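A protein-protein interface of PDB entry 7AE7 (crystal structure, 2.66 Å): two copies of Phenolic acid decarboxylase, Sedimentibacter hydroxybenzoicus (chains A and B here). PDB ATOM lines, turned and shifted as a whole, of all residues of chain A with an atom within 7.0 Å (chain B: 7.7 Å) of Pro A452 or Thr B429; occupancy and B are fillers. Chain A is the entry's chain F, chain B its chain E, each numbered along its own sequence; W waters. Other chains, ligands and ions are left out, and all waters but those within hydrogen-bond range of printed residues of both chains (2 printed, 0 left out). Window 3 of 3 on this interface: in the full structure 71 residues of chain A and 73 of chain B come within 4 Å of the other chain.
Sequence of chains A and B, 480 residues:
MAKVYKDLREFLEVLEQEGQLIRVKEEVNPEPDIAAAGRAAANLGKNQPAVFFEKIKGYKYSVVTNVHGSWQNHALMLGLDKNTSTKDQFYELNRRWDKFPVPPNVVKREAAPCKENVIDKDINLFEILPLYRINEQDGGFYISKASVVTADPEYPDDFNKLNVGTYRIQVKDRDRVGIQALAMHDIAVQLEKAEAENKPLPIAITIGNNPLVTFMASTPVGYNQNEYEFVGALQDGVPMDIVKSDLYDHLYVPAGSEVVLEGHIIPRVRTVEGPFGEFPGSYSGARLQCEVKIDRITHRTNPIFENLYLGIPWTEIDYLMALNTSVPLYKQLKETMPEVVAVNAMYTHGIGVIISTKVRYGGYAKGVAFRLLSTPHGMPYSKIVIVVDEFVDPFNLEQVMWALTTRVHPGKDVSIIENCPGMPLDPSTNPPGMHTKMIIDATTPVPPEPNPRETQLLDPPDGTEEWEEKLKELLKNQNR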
ATOM      1  N   THR A 406     -24.284  -9.547  -8.667  1.00  0.00           N
ATOM      2  CA  THR A 406     -24.224  -9.252  -7.240  1.00  0.00           C
ATOM      3  C   THR A 406     -23.773  -7.833  -6.912  1.00  0.00           C
ATOM      4  O   THR A 406     -23.957  -7.397  -5.770  1.00  0.00           O
ATOM      5  CB  THR A 406     -23.304 -10.249  -6.523  1.00  0.00           C
ATOM      6  OG1 THR A 406     -21.982 -10.165  -7.068  1.00  0.00           O
ATOM      7  CG2 THR A 406     -23.832 -11.669  -6.680  1.00  0.00           C
ATOM      8  N   VAL A 408     -24.022  -4.920  -9.408  1.00  0.00           N
ATOM      9  CA  VAL A 408     -24.560  -3.873 -10.269  1.00  0.00           C
ATOM     10  C   VAL A 408     -25.940  -3.477  -9.764  1.00  0.00           C
ATOM     11  O   VAL A 408     -26.863  -4.299  -9.734  1.00  0.00           O
ATOM     12  CB  VAL A 408     -24.625  -4.327 -11.734  1.00  0.00           C
ATOM     13  CG1 VAL A 408     -25.507  -3.388 -12.544  1.00  0.00           C
ATOM     14  CG2 VAL A 408     -23.240  -4.379 -12.324  1.00  0.00           C
ATOM     15  N   HIS A 409     -26.076  -2.212  -9.372  1.00  0.00           N
ATOM     16  CA  HIS A 409     -27.360  -1.597  -9.082  1.00  0.00           C
ATOM     17  C   HIS A 409     -27.688  -0.706 -10.270  1.00  0.00           C
ATOM     18  O   HIS A 409     -27.101   0.378 -10.404  1.00  0.00           O
ATOM     19  CB  HIS A 409     -27.291  -0.783  -7.784  1.00  0.00           C
ATOM     20  CG  HIS A 409     -28.601  -0.204  -7.343  1.00  0.00           C
ATOM     21  ND1 HIS A 409     -29.557   0.253  -8.226  1.00  0.00           N
ATOM     22  CD2 HIS A 409     -29.109   0.003  -6.104  1.00  0.00           C
ATOM     23  CE1 HIS A 409     -30.595   0.713  -7.551  1.00  0.00           C
ATOM     24  NE2 HIS A 409     -30.349   0.572  -6.262  1.00  0.00           N
ATOM     25  N   PRO A 445     -18.753  -1.351  -3.430  1.00  0.00           N
ATOM     26  CA  PRO A 445     -18.620   0.020  -2.921  1.00  0.00           C
ATOM     27  C   PRO A 445     -17.442   0.161  -1.968  1.00  0.00           C
ATOM     28  O   PRO A 445     -17.173  -0.711  -1.138  1.00  0.00           O
ATOM     29  CB  PRO A 445     -19.955   0.267  -2.209  1.00  0.00           C
ATOM     30  CG  PRO A 445     -20.905  -0.664  -2.865  1.00  0.00           C
ATOM     31  CD  PRO A 445     -20.113  -1.882  -3.233  1.00  0.00           C
ATOM     32  N   GLU A 449     -18.327   5.822  -0.614  1.00  0.00           N
ATOM     33  CA  GLU A 449     -19.591   5.328  -1.156  1.00  0.00           C
ATOM     34  C   GLU A 449     -20.307   4.489  -0.104  1.00  0.00           C
ATOM     35  O   GLU A 449     -19.719   3.532   0.416  1.00  0.00           O
ATOM     36  CB  GLU A 449     -19.354   4.503  -2.417  1.00  0.00           C
ATOM     37  CG  GLU A 449     -20.630   4.008  -3.081  1.00  0.00           C
ATOM     38  CD  GLU A 449     -20.369   3.312  -4.403  1.00  0.00           C
ATOM     39  OE1 GLU A 449     -19.212   3.342  -4.878  1.00  0.00           O
ATOM     40  OE2 GLU A 449     -21.325   2.737  -4.970  1.00  0.00           O
ATOM     41  N   PRO A 450     -21.549   4.814   0.253  1.00  0.00           N
ATOM     42  CA  PRO A 450     -22.284   3.970   1.203  1.00  0.00           C
ATOM     43  C   PRO A 450     -22.494   2.568   0.650  1.00  0.00           C
ATOM     44  O   PRO A 450     -22.725   2.379  -0.545  1.00  0.00           O
ATOM     45  CB  PRO A 450     -23.617   4.708   1.382  1.00  0.00           C
ATOM     46  CG  PRO A 450     -23.352   6.110   0.953  1.00  0.00           C
ATOM     47  CD  PRO A 450     -22.281   6.043  -0.094  1.00  0.00           C
ATOM     48  N   ASN A 451     -22.413   1.583   1.539  1.00  0.00           N
ATOM     49  CA  ASN A 451     -22.623   0.187   1.170  1.00  0.00           C
ATOM     50  C   ASN A 451     -23.934  -0.299   1.769  1.00  0.00           C
ATOM     51  O   ASN A 451     -24.031  -0.435   2.999  1.00  0.00           O
ATOM     52  CB  ASN A 451     -21.459  -0.680   1.650  1.00  0.00           C
ATOM     53  CG  ASN A 451     -21.419  -2.037   0.969  1.00  0.00           C
ATOM     54  OD1 ASN A 451     -22.453  -2.676   0.769  1.00  0.00           O
ATOM     55  ND2 ASN A 451     -20.221  -2.484   0.611  1.00  0.00           N
ATOM     56  N   PRO A 452     -24.961  -0.568   0.957  1.00  0.00           N
ATOM     57  CA  PRO A 452     -26.249  -1.002   1.525  1.00  0.00           C
ATOM     58  C   PRO A 452     -26.160  -2.274   2.349  1.00  0.00           C
ATOM     59  O   PRO A 452     -26.937  -2.436   3.298  1.00  0.00           O
ATOM     60  CB  PRO A 452     -27.140  -1.191   0.287  1.00  0.00           C
ATOM     61  CG  PRO A 452     -26.209  -1.215  -0.885  1.00  0.00           C
ATOM     62  CD  PRO A 452     -25.021  -0.396  -0.503  1.00  0.00           C
ATOM     63  N   ARG A 453     -25.248  -3.194   2.014  1.00  0.00           N
ATOM     64  CA  ARG A 453     -25.053  -4.383   2.843  1.00  0.00           C
ATOM     65  C   ARG A 453     -23.639  -4.914   2.609  1.00  0.00           C
ATOM     66  O   ARG A 453     -23.375  -5.538   1.578  1.00  0.00           O
ATOM     67  CB  ARG A 453     -26.098  -5.444   2.546  1.00  0.00           C
ATOM     68  CG  ARG A 453     -26.133  -6.548   3.584  1.00  0.00           C
ATOM     69  CD  ARG A 453     -27.230  -7.548   3.290  1.00  0.00           C
ATOM     70  NE  ARG A 453     -26.679  -8.821   2.844  1.00  0.00           N
ATOM     71  CZ  ARG A 453     -26.929  -9.371   1.665  1.00  0.00           C
ATOM     72  NH1 ARG A 453     -27.744  -8.797   0.794  1.00  0.00           N
ATOM     73  NH2 ARG A 453     -26.349 -10.525   1.351  1.00  0.00           N
ATOM     74  N   GLU A 454     -22.752  -4.673   3.569  1.00  0.00           N
ATOM     75  CA  GLU A 454     -21.409  -5.228   3.493  1.00  0.00           C
ATOM     76  C   GLU A 454     -21.446  -6.741   3.670  1.00  0.00           C
ATOM     77  O   GLU A 454     -22.205  -7.271   4.488  1.00  0.00           O
ATOM     78  CB  GLU A 454     -20.508  -4.598   4.556  1.00  0.00           C
ATOM     79  N   ILE B 351     -30.506 -14.471 -11.107  1.00  0.00           N
ATOM     80  CA  ILE B 351     -30.477 -13.013 -11.038  1.00  0.00           C
ATOM     81  C   ILE B 351     -30.131 -12.432 -12.403  1.00  0.00           C
ATOM     82  O   ILE B 351     -30.606 -11.349 -12.767  1.00  0.00           O
ATOM     83  CB  ILE B 351     -29.497 -12.546  -9.942  1.00  0.00           C
ATOM     84  CG1 ILE B 351     -30.010 -12.960  -8.563  1.00  0.00           C
ATOM     85  CG2 ILE B 351     -29.316 -11.037  -9.979  1.00  0.00           C
ATOM     86  CD1 ILE B 351     -29.027 -12.698  -7.444  1.00  0.00           C
ATOM     87  N   PRO B 380     -38.997 -11.713  -8.625  1.00  0.00           N
ATOM     88  CA  PRO B 380     -38.142 -11.207  -7.545  1.00  0.00           C
ATOM     89  C   PRO B 380     -36.649 -11.387  -7.795  1.00  0.00           C
ATOM     90  O   PRO B 380     -35.842 -10.611  -7.273  1.00  0.00           O
ATOM     91  CB  PRO B 380     -38.608 -12.022  -6.338  1.00  0.00           C
ATOM     92  CG  PRO B 380     -39.006 -13.323  -6.920  1.00  0.00           C
ATOM     93  CD  PRO B 380     -39.557 -13.038  -8.291  1.00  0.00           C
ATOM     94  N   LYS B 383     -32.700  -9.678 -12.297  1.00  0.00           N
ATOM     95  CA  LYS B 383     -32.377  -8.258 -12.333  1.00  0.00           C
ATOM     96  C   LYS B 383     -31.855  -7.796 -13.682  1.00  0.00           C
ATOM     97  O   LYS B 383     -32.229  -6.718 -14.148  1.00  0.00           O
ATOM     98  CB  LYS B 383     -31.341  -7.932 -11.250  1.00  0.00           C
ATOM     99  CG  LYS B 383     -30.866  -6.490 -11.243  1.00  0.00           C
ATOM    100  CD  LYS B 383     -29.921  -6.237 -10.083  1.00  0.00           C
ATOM    101  CE  LYS B 383     -28.680  -7.111 -10.184  1.00  0.00           C
ATOM    102  NZ  LYS B 383     -27.628  -6.701  -9.213  1.00  0.00           N
ATOM    103  N   PRO B 421     -39.807  -5.716  -7.704  1.00  0.00           N
ATOM    104  CA  PRO B 421     -39.505  -6.747  -6.706  1.00  0.00           C
ATOM    105  C   PRO B 421     -38.035  -7.132  -6.751  1.00  0.00           C
ATOM    106  O   PRO B 421     -37.431  -7.229  -7.820  1.00  0.00           O
ATOM    107  CB  PRO B 421     -40.400  -7.919  -7.122  1.00  0.00           C
ATOM    108  CG  PRO B 421     -41.506  -7.297  -7.893  1.00  0.00           C
ATOM    109  CD  PRO B 421     -40.883  -6.141  -8.618  1.00  0.00           C
ATOM    110  N   GLY B 422     -37.467  -7.356  -5.573  1.00  0.00           N
ATOM    111  CA  GLY B 422     -36.080  -7.756  -5.479  1.00  0.00           C
ATOM    112  C   GLY B 422     -35.899  -8.931  -4.547  1.00  0.00           C
ATOM    113  O   GLY B 422     -36.871  -9.599  -4.179  1.00  0.00           O
ATOM    114  N   MET B 423     -34.655  -9.193  -4.153  1.00  0.00           N
ATOM    115  CA  MET B 423     -34.377 -10.296  -3.266  1.00  0.00           C
ATOM    116  C   MET B 423     -33.206  -9.910  -2.379  1.00  0.00           C
ATOM    117  O   MET B 423     -32.223  -9.344  -2.879  1.00  0.00           O
ATOM    118  CB  MET B 423     -34.065 -11.573  -4.046  1.00  0.00           C
ATOM    119  CG  MET B 423     -35.270 -12.462  -4.308  1.00  0.00           C
ATOM    120  SD  MET B 423     -35.949 -13.145  -2.787  1.00  0.00           S
ATOM    121  CE  MET B 423     -37.698 -13.151  -3.156  1.00  0.00           C
ATOM    122  N   PRO B 424     -33.284 -10.182  -1.075  1.00  0.00           N
ATOM    123  CA  PRO B 424     -32.201  -9.759  -0.171  1.00  0.00           C
ATOM    124  C   PRO B 424     -30.853 -10.377  -0.498  1.00  0.00           C
ATOM    125  O   PRO B 424     -29.817  -9.785  -0.166  1.00  0.00           O
ATOM    126  CB  PRO B 424     -32.701 -10.200   1.212  1.00  0.00           C
ATOM    127  CG  PRO B 424     -34.176 -10.397   1.056  1.00  0.00           C
ATOM    128  CD  PRO B 424     -34.391 -10.833  -0.358  1.00  0.00           C
ATOM    129  N   LEU B 425     -30.831 -11.544  -1.148  1.00  0.00           N
ATOM    130  CA  LEU B 425     -29.571 -12.225  -1.424  1.00  0.00           C
ATOM    131  C   LEU B 425     -28.665 -11.412  -2.342  1.00  0.00           C
ATOM    132  O   LEU B 425     -27.463 -11.695  -2.417  1.00  0.00           O
ATOM    133  CB  LEU B 425     -29.840 -13.603  -2.034  1.00  0.00           C
ATOM    134  CG  LEU B 425     -29.823 -13.739  -3.559  1.00  0.00           C
ATOM    135  CD1 LEU B 425     -29.842 -15.194  -3.940  1.00  0.00           C
ATOM    136  CD2 LEU B 425     -30.994 -13.033  -4.190  1.00  0.00           C
ATOM    137  N   ASP B 426     -29.212 -10.418  -3.044  1.00  0.00           N
ATOM    138  CA  ASP B 426     -28.433  -9.480  -3.842  1.00  0.00           C
ATOM    139  C   ASP B 426     -27.913  -8.382  -2.922  1.00  0.00           C
ATOM    140  O   ASP B 426     -28.689  -7.533  -2.464  1.00  0.00           O
ATOM    141  CB  ASP B 426     -29.292  -8.898  -4.969  1.00  0.00           C
ATOM    142  CG  ASP B 426     -28.528  -7.935  -5.877  1.00  0.00           C
ATOM    143  OD1 ASP B 426     -27.432  -7.459  -5.507  1.00  0.00           O
ATOM    144  OD2 ASP B 426     -29.045  -7.642  -6.976  1.00  0.00           O
ATOM    145  N   PRO B 427     -26.610  -8.361  -2.631  1.00  0.00           N
ATOM    146  CA  PRO B 427     -26.083  -7.347  -1.702  1.00  0.00           C
ATOM    147  C   PRO B 427     -26.186  -5.925  -2.220  1.00  0.00           C
ATOM    148  O   PRO B 427     -26.197  -4.989  -1.411  1.00  0.00           O
ATOM    149  CB  PRO B 427     -24.621  -7.773  -1.513  1.00  0.00           C
ATOM    150  CG  PRO B 427     -24.291  -8.537  -2.754  1.00  0.00           C
ATOM    151  CD  PRO B 427     -25.553  -9.246  -3.149  1.00  0.00           C
ATOM    152  N   SER B 428     -26.276  -5.727  -3.534  1.00  0.00           N
ATOM    153  CA  SER B 428     -26.262  -4.388  -4.109  1.00  0.00           C
ATOM    154  C   SER B 428     -27.635  -3.729  -4.136  1.00  0.00           C
ATOM    155  O   SER B 428     -27.739  -2.578  -4.574  1.00  0.00           O
ATOM    156  CB  SER B 428     -25.685  -4.433  -5.527  1.00  0.00           C
ATOM    157  OG  SER B 428     -26.648  -4.895  -6.458  1.00  0.00           O
ATOM    158  N   THR B 429     -28.683  -4.420  -3.692  1.00  0.00           N
ATOM    159  CA  THR B 429     -30.020  -3.841  -3.710  1.00  0.00           C
ATOM    160  C   THR B 429     -30.116  -2.681  -2.726  1.00  0.00           C
ATOM    161  O   THR B 429     -29.705  -2.798  -1.567  1.00  0.00           O
ATOM    162  CB  THR B 429     -31.068  -4.904  -3.376  1.00  0.00           C
ATOM    163  OG1 THR B 429     -30.738  -5.544  -2.137  1.00  0.00           O
ATOM    164  CG2 THR B 429     -31.143  -5.943  -4.478  1.00  0.00           C
ATOM    165  N   ASN B 430     -30.666  -1.561  -3.192  1.00  0.00           N
ATOM    166  CA  ASN B 430     -30.888  -0.388  -2.356  1.00  0.00           C
ATOM    167  C   ASN B 430     -32.142   0.341  -2.830  1.00  0.00           C
ATOM    168  O   ASN B 430     -32.122   0.976  -3.892  1.00  0.00           O
ATOM    169  CB  ASN B 430     -29.675   0.543  -2.387  1.00  0.00           C
ATOM    170  CG  ASN B 430     -29.692   1.556  -1.262  1.00  0.00           C
ATOM    171  OD1 ASN B 430     -30.626   1.595  -0.462  1.00  0.00           O
ATOM    172  ND2 ASN B 430     -28.657   2.384  -1.196  1.00  0.00           N
ATOM    173  N   PRO B 431     -33.257   0.280  -2.079  1.00  0.00           N
ATOM    174  CA  PRO B 431     -33.398  -0.332  -0.751  1.00  0.00           C
ATOM    175  C   PRO B 431     -33.254  -1.851  -0.782  1.00  0.00           C
ATOM    176  O   PRO B 431     -33.611  -2.465  -1.789  1.00  0.00           O
ATOM    177  CB  PRO B 431     -34.819   0.065  -0.315  1.00  0.00           C
ATOM    178  CG  PRO B 431     -35.356   0.968  -1.385  1.00  0.00           C
ATOM    179  CD  PRO B 431     -34.550   0.738  -2.612  1.00  0.00           C
ATOM    180  N   PRO B 432     -32.720  -2.435   0.290  1.00  0.00           N
ATOM    181  CA  PRO B 432     -32.486  -3.884   0.298  1.00  0.00           C
ATOM    182  C   PRO B 432     -33.771  -4.654   0.037  1.00  0.00           C
ATOM    183  O   PRO B 432     -34.842  -4.302   0.534  1.00  0.00           O
ATOM    184  CB  PRO B 432     -31.946  -4.149   1.708  1.00  0.00           C
ATOM    185  CG  PRO B 432     -31.339  -2.847   2.121  1.00  0.00           C
ATOM    186  CD  PRO B 432     -32.202  -1.781   1.504  1.00  0.00           C
ATOM    187  N   GLY B 433     -33.654  -5.709  -0.766  1.00  0.00           N
ATOM    188  CA  GLY B 433     -34.799  -6.501  -1.151  1.00  0.00           C
ATOM    189  C   GLY B 433     -35.632  -5.920  -2.269  1.00  0.00           C
ATOM    190  O   GLY B 433     -36.644  -6.527  -2.643  1.00  0.00           O
ATOM    191  N   MET B 434     -35.252  -4.763  -2.806  1.00  0.00           N
ATOM    192  CA  MET B 434     -35.924  -4.149  -3.941  1.00  0.00           C
ATOM    193  C   MET B 434     -34.958  -4.083  -5.113  1.00  0.00           C
ATOM    194  O   MET B 434     -33.740  -3.993  -4.932  1.00  0.00           O
ATOM    195  CB  MET B 434     -36.432  -2.739  -3.604  1.00  0.00           C
ATOM    196  CG  MET B 434     -37.492  -2.700  -2.515  1.00  0.00           C
ATOM    197  SD  MET B 434     -39.114  -3.258  -3.075  1.00  0.00           S
ATOM    198  CE  MET B 434     -39.459  -2.068  -4.373  1.00  0.00           C
ATOM    199  N   HIS B 435     -35.505  -4.124  -6.322  1.00  0.00           N
ATOM    200  CA  HIS B 435     -34.690  -4.142  -7.522  1.00  0.00           C
ATOM    201  C   HIS B 435     -34.966  -2.929  -8.395  1.00  0.00           C
ATOM    202  O   HIS B 435     -36.083  -2.403  -8.438  1.00  0.00           O
ATOM    203  CB  HIS B 435     -34.931  -5.405  -8.355  1.00  0.00           C
ATOM    204  CG  HIS B 435     -33.959  -6.507  -8.078  1.00  0.00           C
ATOM    205  ND1 HIS B 435     -34.237  -7.830  -8.349  1.00  0.00           N
ATOM    206  CD2 HIS B 435     -32.714  -6.485  -7.549  1.00  0.00           C
ATOM    207  CE1 HIS B 435     -33.203  -8.574  -8.001  1.00  0.00           C
ATOM    208  NE2 HIS B 435     -32.265  -7.783  -7.512  1.00  0.00           N
ATOM    209  N   THR B 436     -33.924  -2.500  -9.087  1.00  0.00           N
ATOM    210  CA  THR B 436     -34.046  -1.680 -10.283  1.00  0.00           C
ATOM    211  C   THR B 436     -33.659  -2.615 -11.427  1.00  0.00           C
ATOM    212  O   THR B 436     -32.484  -2.942 -11.603  1.00  0.00           O
ATOM    213  CB  THR B 436     -33.160  -0.441 -10.202  1.00  0.00           C
ATOM    214  OG1 THR B 436     -33.588   0.380  -9.110  1.00  0.00           O
ATOM    215  CG2 THR B 436     -33.285   0.362 -11.459  1.00  0.00           C
HETATM  216  O   HOH W   1     -32.294  -1.990  -5.556  1.00  0.00           O
HETATM  217  O   HOH W   2     -29.446  -6.913   0.948  1.00  0.00           O
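NZ of Lys B383 sits at hydrogen-bond distance from O of Val A408. O of Pro B424 sits at hydrogen-bond distance from NH1 of Arg A453, at 2.5 Å. The side-chain hydroxyl (OG) of Ser B428 sits at hydrogen-bond distance from the backbone carbonyl oxygen (O) of Val A408 (3.3 Å). O of Asn B430 is in hydrogen-bond range of NE2 of His A409, 3.0 Å away. The backbone carbonyl oxygen of Thr A406 lies close to the side-chain carboxylate of Asp B426, at 3.5 Å.
No position is printed for both chains.
Hydrophobic or aromatic side chains of chain B that line the printed part of chain A: Pro B427. Hydrophobic or aromatic side chains of chain A that line the printed part of chain B: His A409 and Pro A452. Among the printed residues, 13 pairs touch across the chains. Among the printed residues, no Asp or Glu carboxylate lies within 4 Å of a Lys or Arg side-chain nitrogen of the other chain.
The backbone carbonyl oxygen (O) of Ile B351 sits at hydrogen-bond distance from the backbone NH (N) of Lys B383 (2.7 Å). The side-chain amino group (NZ) of Lys B383 is in salt-bridge range of the side-chain carboxylate (OD2) of Asp B426, at 2.8 Å. The side-chain amino group of Lys B383 is in hydrogen-bond range of the side-chain hydroxyl of Ser B428, 3.4 Å away. The side-chain hydroxyl of Thr B429 sits at hydrogen-bond distance from the backbone carbonyl oxygen of Asp B426, at 2.9 Å. NE2 of His B435 is in hydrogen-bond range of OD2 of Asp B426. The backbone NH (N) of Gly B433 sits at hydrogen-bond distance from the side-chain hydroxyl (OG1) of Thr B429.
Among the printed residues, merely in contact across the chains: Thr A406 with Pro B427, His A409 with Ser B428, Arg A453 with Pro B427, His A409 with Thr B436, Thr A406 with Ser B428, Pro A452 with Thr B429, Arg A453 with Asp B426 and Pro A452 with Pro B427.
Printed residues of chain B within 4 Å of His A409: Ser B428 (3.3 Å), Asn B430 (3.0 Å) and Thr B436 (3.4 Å). Asn A451 touches none of the printed residues of chain B. Of chain B, only Pro B427 (3.8 Å) and Thr B429 (3.5 Å) come within 4 Å of Pro A452. Of the printed residues of chain A, Pro B424 touches Arg A453 (2.5 Å). Of chain A, only Pro A452 comes within 4 Å of Thr B429. Pro B432 touches none of the printed residues of chain A. Of the printed residues of chain A, Thr B436 touches His A409. The nearest residue of chain A that does not touch Thr B429 is His A409 (4.4 Å). The nearest printed residue of chain A that does not touch Ser B428 is Pro A452 (4.2 Å).
Water W2 lies within hydrogen-bond range of the guanidinium group of Arg A453 (2.5 Å) and the backbone carbonyl oxygen of Pro B424 (3.1 Å). Water W1 lies within hydrogen-bond range of the backbone carbonyl oxygen of Met B434 (2.5 Å), the backbone NH of Asn B430 (2.9 Å) and a ring nitrogen (NE2) of His A409 (3.3 Å).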
